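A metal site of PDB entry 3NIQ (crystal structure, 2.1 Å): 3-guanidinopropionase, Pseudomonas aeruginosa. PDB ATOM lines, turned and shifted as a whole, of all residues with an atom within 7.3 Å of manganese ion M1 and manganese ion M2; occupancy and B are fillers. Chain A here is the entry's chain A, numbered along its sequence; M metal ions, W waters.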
ATOM      1  N   ASP A 125      23.096 -12.761 -10.238  1.00  0.00           N
ATOM      2  CA  ASP A 125      21.650 -12.890 -10.177  1.00  0.00           C
ATOM      3  C   ASP A 125      21.055 -12.638 -11.563  1.00  0.00           C
ATOM      4  O   ASP A 125      21.775 -12.309 -12.508  1.00  0.00           O
ATOM      5  CB  ASP A 125      21.068 -11.961  -9.099  1.00  0.00           C
ATOM      6  CG  ASP A 125      21.145 -10.467  -9.489  1.00  0.00           C
ATOM      7  OD1 ASP A 125      21.177 -10.122 -10.682  1.00  0.00           O
ATOM      8  OD2 ASP A 125      21.178  -9.629  -8.571  1.00  0.00           O
ATOM      9  N   HIS A 126      19.740 -12.756 -11.699  1.00  0.00           N
ATOM     10  CA  HIS A 126      19.131 -12.788 -13.034  1.00  0.00           C
ATOM     11  C   HIS A 126      19.140 -11.424 -13.743  1.00  0.00           C
ATOM     12  O   HIS A 126      18.922 -11.349 -14.957  1.00  0.00           O
ATOM     13  CB  HIS A 126      17.705 -13.338 -12.986  1.00  0.00           C
ATOM     14  CG  HIS A 126      17.425 -14.311 -14.079  1.00  0.00           C
ATOM     15  ND1 HIS A 126      16.646 -15.439 -13.890  1.00  0.00           N
ATOM     16  CD2 HIS A 126      17.880 -14.376 -15.350  1.00  0.00           C
ATOM     17  CE1 HIS A 126      16.617 -16.138 -15.012  1.00  0.00           C
ATOM     18  NE2 HIS A 126      17.366 -15.521 -15.914  1.00  0.00           N
ATOM     19  N   LEU A 127      19.441 -10.354 -13.006  1.00  0.00           N
ATOM     20  CA  LEU A 127      19.532  -9.038 -13.657  1.00  0.00           C
ATOM     21  C   LEU A 127      20.665  -9.017 -14.673  1.00  0.00           C
ATOM     22  O   LEU A 127      20.629  -8.265 -15.647  1.00  0.00           O
ATOM     23  CB  LEU A 127      19.646  -7.890 -12.626  1.00  0.00           C
ATOM     24  CG  LEU A 127      19.720  -6.481 -13.238  1.00  0.00           C
ATOM     25  CD1 LEU A 127      18.444  -6.174 -14.063  1.00  0.00           C
ATOM     26  CD2 LEU A 127      19.945  -5.380 -12.154  1.00  0.00           C
ATOM     27  N   HIS A 146      13.081 -20.111 -20.740  1.00  0.00           N
ATOM     28  CA  HIS A 146      13.496 -19.576 -19.455  1.00  0.00           C
ATOM     29  C   HIS A 146      13.013 -20.524 -18.341  1.00  0.00           C
ATOM     30  O   HIS A 146      11.811 -20.720 -18.161  1.00  0.00           O
ATOM     31  CB  HIS A 146      12.860 -18.182 -19.321  1.00  0.00           C
ATOM     32  CG  HIS A 146      13.018 -17.545 -17.975  1.00  0.00           C
ATOM     33  ND1 HIS A 146      12.068 -16.703 -17.436  1.00  0.00           N
ATOM     34  CD2 HIS A 146      14.028 -17.613 -17.061  1.00  0.00           C
ATOM     35  CE1 HIS A 146      12.461 -16.297 -16.246  1.00  0.00           C
ATOM     36  NE2 HIS A 146      13.651 -16.830 -15.994  1.00  0.00           N
ATOM     37  N   PHE A 147      13.944 -21.135 -17.637  1.00  0.00           N
ATOM     38  CA  PHE A 147      13.652 -22.064 -16.529  1.00  0.00           C
ATOM     39  C   PHE A 147      13.761 -21.294 -15.212  1.00  0.00           C
ATOM     40  O   PHE A 147      14.837 -20.758 -14.920  1.00  0.00           O
ATOM     41  CB  PHE A 147      14.691 -23.197 -16.501  1.00  0.00           C
ATOM     42  CG  PHE A 147      14.671 -24.056 -17.722  1.00  0.00           C
ATOM     43  CD1 PHE A 147      13.918 -25.217 -17.756  1.00  0.00           C
ATOM     44  CD2 PHE A 147      15.446 -23.724 -18.833  1.00  0.00           C
ATOM     45  CE1 PHE A 147      13.910 -26.037 -18.894  1.00  0.00           C
ATOM     46  CE2 PHE A 147      15.438 -24.525 -19.966  1.00  0.00           C
ATOM     47  CZ  PHE A 147      14.675 -25.686 -19.999  1.00  0.00           C
ATOM     48  N   ASP A 148      12.687 -21.218 -14.442  1.00  0.00           N
ATOM     49  CA  ASP A 148      12.694 -20.373 -13.245  1.00  0.00           C
ATOM     50  C   ASP A 148      11.525 -20.690 -12.315  1.00  0.00           C
ATOM     51  O   ASP A 148      10.439 -21.087 -12.777  1.00  0.00           O
ATOM     52  CB  ASP A 148      12.612 -18.893 -13.686  1.00  0.00           C
ATOM     53  CG  ASP A 148      13.270 -17.928 -12.701  1.00  0.00           C
ATOM     54  OD1 ASP A 148      13.055 -18.021 -11.472  1.00  0.00           O
ATOM     55  OD2 ASP A 148      13.989 -17.033 -13.175  1.00  0.00           O
ATOM     56  N   ALA A 149      11.731 -20.510 -11.008  1.00  0.00           N
ATOM     57  CA  ALA A 149      10.593 -20.507 -10.080  1.00  0.00           C
ATOM     58  C   ALA A 149       9.786 -19.196 -10.203  1.00  0.00           C
ATOM     59  O   ALA A 149       8.646 -19.134  -9.720  1.00  0.00           O
ATOM     60  CB  ALA A 149      11.064 -20.710  -8.639  1.00  0.00           C
ATOM     61  N   HIS A 150      10.378 -18.177 -10.821  1.00  0.00           N
ATOM     62  CA  HIS A 150       9.777 -16.825 -10.916  1.00  0.00           C
ATOM     63  C   HIS A 150       9.774 -16.260 -12.346  1.00  0.00           C
ATOM     64  O   HIS A 150      10.721 -16.442 -13.103  1.00  0.00           O
ATOM     65  CB  HIS A 150      10.534 -15.841 -10.006  1.00  0.00           C
ATOM     66  CG  HIS A 150      10.877 -16.408  -8.665  1.00  0.00           C
ATOM     67  ND1 HIS A 150      12.103 -16.999  -8.393  1.00  0.00           N
ATOM     68  CD2 HIS A 150      10.163 -16.473  -7.511  1.00  0.00           C
ATOM     69  CE1 HIS A 150      12.113 -17.422  -7.145  1.00  0.00           C
ATOM     70  NE2 HIS A 150      10.959 -17.102  -6.579  1.00  0.00           N
ATOM     71  N   SER A 151       8.723 -15.524 -12.702  1.00  0.00           N
ATOM     72  CA  SER A 151       8.663 -14.950 -14.047  1.00  0.00           C
ATOM     73  C   SER A 151       9.679 -13.847 -14.273  1.00  0.00           C
ATOM     74  O   SER A 151      10.107 -13.625 -15.419  1.00  0.00           O
ATOM     75  CB  SER A 151       7.241 -14.470 -14.359  1.00  0.00           C
ATOM     76  OG  SER A 151       6.866 -13.427 -13.483  1.00  0.00           O
ATOM     77  N   ASP A 152      10.074 -13.128 -13.207  1.00  0.00           N
ATOM     78  CA  ASP A 152      11.058 -12.033 -13.324  1.00  0.00           C
ATOM     79  C   ASP A 152      10.576 -10.961 -14.304  1.00  0.00           C
ATOM     80  O   ASP A 152      11.356 -10.406 -15.092  1.00  0.00           O
ATOM     81  CB  ASP A 152      12.432 -12.554 -13.815  1.00  0.00           C
ATOM     82  CG  ASP A 152      13.128 -13.432 -12.797  1.00  0.00           C
ATOM     83  OD1 ASP A 152      12.655 -13.498 -11.653  1.00  0.00           O
ATOM     84  OD2 ASP A 152      14.143 -14.079 -13.146  1.00  0.00           O
ATOM     85  N   HIS A 165      16.786  -8.191  -9.988  1.00  0.00           N
ATOM     86  CA  HIS A 165      16.786  -9.544 -10.538  1.00  0.00           C
ATOM     87  C   HIS A 165      15.356 -10.026 -10.818  1.00  0.00           C
ATOM     88  O   HIS A 165      15.161 -11.051 -11.456  1.00  0.00           O
ATOM     89  CB  HIS A 165      17.549 -10.510  -9.619  1.00  0.00           C
ATOM     90  CG  HIS A 165      16.910 -10.721  -8.277  1.00  0.00           C
ATOM     91  ND1 HIS A 165      17.200 -11.813  -7.481  1.00  0.00           N
ATOM     92  CD2 HIS A 165      15.995  -9.990  -7.596  1.00  0.00           C
ATOM     93  CE1 HIS A 165      16.508 -11.726  -6.352  1.00  0.00           C
ATOM     94  NE2 HIS A 165      15.759 -10.631  -6.408  1.00  0.00           N
ATOM     95  N   GLY A 166      14.355  -9.275 -10.359  1.00  0.00           N
ATOM     96  CA  GLY A 166      12.957  -9.611 -10.604  1.00  0.00           C
ATOM     97  C   GLY A 166      12.307  -8.825 -11.739  1.00  0.00           C
ATOM     98  O   GLY A 166      11.142  -9.041 -12.022  1.00  0.00           O
ATOM     99  N   PRO A 168      14.108  -8.253 -15.048  1.00  0.00           N
ATOM    100  CA  PRO A 168      14.886  -8.131 -16.302  1.00  0.00           C
ATOM    101  C   PRO A 168      14.089  -8.411 -17.589  1.00  0.00           C
ATOM    102  O   PRO A 168      14.342  -7.783 -18.615  1.00  0.00           O
ATOM    103  CB  PRO A 168      16.008  -9.142 -16.118  1.00  0.00           C
ATOM    104  CG  PRO A 168      15.425 -10.200 -15.207  1.00  0.00           C
ATOM    105  CD  PRO A 168      14.564  -9.402 -14.243  1.00  0.00           C
ATOM    106  N   PHE A 169      13.180  -9.371 -17.552  1.00  0.00           N
ATOM    107  CA  PHE A 169      12.506  -9.751 -18.783  1.00  0.00           C
ATOM    108  C   PHE A 169      11.378  -8.806 -19.142  1.00  0.00           C
ATOM    109  O   PHE A 169      10.984  -8.720 -20.313  1.00  0.00           O
ATOM    110  CB  PHE A 169      12.098 -11.237 -18.745  1.00  0.00           C
ATOM    111  CG  PHE A 169      13.278 -12.129 -18.621  1.00  0.00           C
ATOM    112  CD1 PHE A 169      13.416 -12.996 -17.538  1.00  0.00           C
ATOM    113  CD2 PHE A 169      14.335 -12.013 -19.525  1.00  0.00           C
ATOM    114  CE1 PHE A 169      14.566 -13.780 -17.391  1.00  0.00           C
ATOM    115  CE2 PHE A 169      15.482 -12.782 -19.394  1.00  0.00           C
ATOM    116  CZ  PHE A 169      15.602 -13.672 -18.303  1.00  0.00           C
ATOM    117  N   SER A 238      17.893 -19.307 -20.732  1.00  0.00           N
ATOM    118  CA  SER A 238      18.314 -18.776 -19.470  1.00  0.00           C
ATOM    119  C   SER A 238      17.833 -19.688 -18.337  1.00  0.00           C
ATOM    120  O   SER A 238      16.633 -19.897 -18.149  1.00  0.00           O
ATOM    121  CB  SER A 238      17.762 -17.359 -19.313  1.00  0.00           C
ATOM    122  OG  SER A 238      18.169 -16.811 -18.075  1.00  0.00           O
ATOM    123  N   PHE A 239      18.784 -20.186 -17.552  1.00  0.00           N
ATOM    124  CA  PHE A 239      18.481 -21.177 -16.523  1.00  0.00           C
ATOM    125  C   PHE A 239      18.753 -20.622 -15.113  1.00  0.00           C
ATOM    126  O   PHE A 239      19.913 -20.411 -14.736  1.00  0.00           O
ATOM    127  CB  PHE A 239      19.336 -22.436 -16.782  1.00  0.00           C
ATOM    128  CG  PHE A 239      18.950 -23.607 -15.925  1.00  0.00           C
ATOM    129  CD1 PHE A 239      18.012 -24.536 -16.379  1.00  0.00           C
ATOM    130  CD2 PHE A 239      19.513 -23.784 -14.660  1.00  0.00           C
ATOM    131  CE1 PHE A 239      17.635 -25.640 -15.578  1.00  0.00           C
ATOM    132  CE2 PHE A 239      19.138 -24.861 -13.842  1.00  0.00           C
ATOM    133  CZ  PHE A 239      18.200 -25.790 -14.297  1.00  0.00           C
ATOM    134  N   ASP A 240      17.682 -20.375 -14.360  1.00  0.00           N
ATOM    135  CA  ASP A 240      17.797 -19.898 -12.998  1.00  0.00           C
ATOM    136  C   ASP A 240      17.730 -21.170 -12.128  1.00  0.00           C
ATOM    137  O   ASP A 240      16.756 -21.913 -12.199  1.00  0.00           O
ATOM    138  CB  ASP A 240      16.652 -18.904 -12.699  1.00  0.00           C
ATOM    139  CG  ASP A 240      16.627 -18.395 -11.253  1.00  0.00           C
ATOM    140  OD1 ASP A 240      17.197 -19.046 -10.341  1.00  0.00           O
ATOM    141  OD2 ASP A 240      15.990 -17.347 -10.994  1.00  0.00           O
ATOM    142  N   VAL A 241      18.783 -21.418 -11.354  1.00  0.00           N
ATOM    143  CA  VAL A 241      18.884 -22.672 -10.634  1.00  0.00           C
ATOM    144  C   VAL A 241      17.767 -22.821  -9.604  1.00  0.00           C
ATOM    145  O   VAL A 241      17.480 -23.926  -9.187  1.00  0.00           O
ATOM    146  CB  VAL A 241      20.265 -22.907  -9.965  1.00  0.00           C
ATOM    147  CG1 VAL A 241      21.406 -22.983 -11.008  1.00  0.00           C
ATOM    148  CG2 VAL A 241      20.558 -21.843  -8.902  1.00  0.00           C
ATOM    149  N   ASP A 242      17.118 -21.723  -9.224  1.00  0.00           N
ATOM    150  CA  ASP A 242      15.997 -21.838  -8.279  1.00  0.00           C
ATOM    151  C   ASP A 242      14.724 -22.460  -8.928  1.00  0.00           C
ATOM    152  O   ASP A 242      13.726 -22.693  -8.246  1.00  0.00           O
ATOM    153  CB  ASP A 242      15.747 -20.496  -7.521  1.00  0.00           C
ATOM    154  CG  ASP A 242      15.041 -19.432  -8.381  1.00  0.00           C
ATOM    155  OD1 ASP A 242      14.411 -19.768  -9.396  1.00  0.00           O
ATOM    156  OD2 ASP A 242      15.119 -18.231  -8.001  1.00  0.00           O
ATOM    157  N   VAL A 243      14.766 -22.758 -10.236  1.00  0.00           N
ATOM    158  CA  VAL A 243      13.739 -23.623 -10.847  1.00  0.00           C
ATOM    159  C   VAL A 243      13.765 -25.009 -10.171  1.00  0.00           C
ATOM    160  O   VAL A 243      12.737 -25.672 -10.001  1.00  0.00           O
ATOM    161  CB  VAL A 243      13.925 -23.793 -12.364  1.00  0.00           C
ATOM    162  CG1 VAL A 243      15.125 -24.688 -12.687  1.00  0.00           C
ATOM    163  CG2 VAL A 243      12.630 -24.311 -13.013  1.00  0.00           C
ATOM    164  N   THR A 252      20.882 -20.716  -3.352  1.00  0.00           N
ATOM    165  CA  THR A 252      20.238 -19.743  -4.226  1.00  0.00           C
ATOM    166  C   THR A 252      19.484 -18.728  -3.379  1.00  0.00           C
ATOM    167  O   THR A 252      19.025 -19.036  -2.261  1.00  0.00           O
ATOM    168  CB  THR A 252      19.319 -20.429  -5.268  1.00  0.00           C
ATOM    169  OG1 THR A 252      19.059 -19.529  -6.353  1.00  0.00           O
ATOM    170  CG2 THR A 252      17.999 -20.907  -4.620  1.00  0.00           C
ATOM    171  N   THR A 254      16.580 -16.955  -3.672  1.00  0.00           N
ATOM    172  CA  THR A 254      15.122 -16.963  -3.481  1.00  0.00           C
ATOM    173  C   THR A 254      14.523 -18.364  -3.671  1.00  0.00           C
ATOM    174  O   THR A 254      13.786 -18.606  -4.642  1.00  0.00           O
ATOM    175  CB  THR A 254      14.452 -15.954  -4.446  1.00  0.00           C
ATOM    176  OG1 THR A 254      15.098 -14.687  -4.302  1.00  0.00           O
ATOM    177  CG2 THR A 254      12.940 -15.783  -4.113  1.00  0.00           C
ATOM    178  N   GLU A 256      12.208 -21.673  -3.528  1.00  0.00           N
ATOM    179  CA  GLU A 256      10.787 -21.985  -3.405  1.00  0.00           C
ATOM    180  C   GLU A 256      10.686 -23.504  -3.417  1.00  0.00           C
ATOM    181  O   GLU A 256      11.171 -24.137  -4.356  1.00  0.00           O
ATOM    182  CB  GLU A 256       9.990 -21.437  -4.612  1.00  0.00           C
ATOM    183  CG  GLU A 256      10.226 -19.957  -4.960  1.00  0.00           C
ATOM    184  CD  GLU A 256       9.554 -18.997  -3.994  1.00  0.00           C
ATOM    185  OE1 GLU A 256       8.715 -19.454  -3.179  1.00  0.00           O
ATOM    186  OE2 GLU A 256       9.854 -17.772  -4.055  1.00  0.00           O
ATOM    187  N   VAL A 283      22.083 -18.817 -13.939  1.00  0.00           N
ATOM    188  CA  VAL A 283      22.154 -17.697 -12.992  1.00  0.00           C
ATOM    189  C   VAL A 283      21.646 -18.104 -11.620  1.00  0.00           C
ATOM    190  O   VAL A 283      21.059 -19.158 -11.485  1.00  0.00           O
ATOM    191  CB  VAL A 283      21.339 -16.489 -13.499  1.00  0.00           C
ATOM    192  CG1 VAL A 283      21.927 -15.980 -14.793  1.00  0.00           C
ATOM    193  CG2 VAL A 283      19.825 -16.850 -13.648  1.00  0.00           C
ATOM    194  N   GLU A 284      21.933 -17.247 -10.634  1.00  0.00           N
ATOM    195  CA  GLU A 284      21.440 -17.329  -9.239  1.00  0.00           C
ATOM    196  C   GLU A 284      22.134 -18.420  -8.395  1.00  0.00           C
ATOM    197  O   GLU A 284      21.651 -18.732  -7.296  1.00  0.00           O
ATOM    198  CB  GLU A 284      19.886 -17.461  -9.161  1.00  0.00           C
ATOM    199  CG  GLU A 284      19.089 -16.282  -9.753  1.00  0.00           C
ATOM    200  CD  GLU A 284      19.188 -14.999  -8.912  1.00  0.00           C
ATOM    201  OE1 GLU A 284      19.827 -15.002  -7.834  1.00  0.00           O
ATOM    202  OE2 GLU A 284      18.651 -13.967  -9.358  1.00  0.00           O
HETATM  203 MN    MN M   1      15.315 -15.621 -12.118  1.00  0.00          MN
HETATM  204 MN    MN M   2      14.048 -17.326  -9.778  1.00  0.00          MN
HETATM  205  O   HOH W   1      13.985 -15.127 -10.161  1.00  0.00           O
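The side-chain carboxylate (OE2) of Glu 256 lies within hydrogen-bond range of a ring nitrogen (NE2) of His 150.
The backbone carbonyl oxygen of Asp 152 lies within hydrogen-bond range of the backbone NH of Phe 169, at 3.2 Å.
The backbone NH of Asp 240 lies within hydrogen-bond range of the backbone carbonyl oxygen of Phe 147 (2.9 Å).
NE2 of His 146 lies close to OD2 of Asp 148 (2.8 Å).
The side-chain carboxylate of Asp 242 sits close to the backbone NH of Ala 149 (3.2 Å).
A ring nitrogen (NE2) of His 126 sits at hydrogen-bond distance from the side-chain hydroxyl (OG) of Ser 238 (2.6 Å).
The backbone NH (N) of His 126 lies within hydrogen-bond range of the side-chain carboxylate (OE2) of Glu 284, 2.9 Å away.
Within 4 Å of manganese ion M1: His 126, Asp 148, Asp 152 and Asp 240.
The nearest printed residue that does not touch manganese ion M1 is His 146 (4.4 Å).
Of the 25 residues printed, 4 come within 4 Å of manganese ion M2.
Manganese ion M1 is bound by the side-chain carboxylate (OD2) of Asp 240.
OD2 of Asp 152 is bound to manganese ion M1 (2.2 Å).
OD2 of Asp 148 is bound to manganese ion M1 (2.2 Å).
ND1 of His 126 binds manganese ion M1 (2.2 Å).
Manganese ion M1 is bound by water W1 (2.4 Å).
Manganese ion M1 has five donor atoms within binding distance.
Manganese ion M2 is bound by the side-chain carboxylate (OD1) of Asp 148, water W1, the side-chain carboxylate (OD2) of Asp 242, the side-chain carboxylate (OD2) of Asp 240, a ring nitrogen (ND1) of His 150 and the side-chain carboxylate (OD1) of Asp 242.
Manganese ion M2 has six donor atoms within binding distance.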
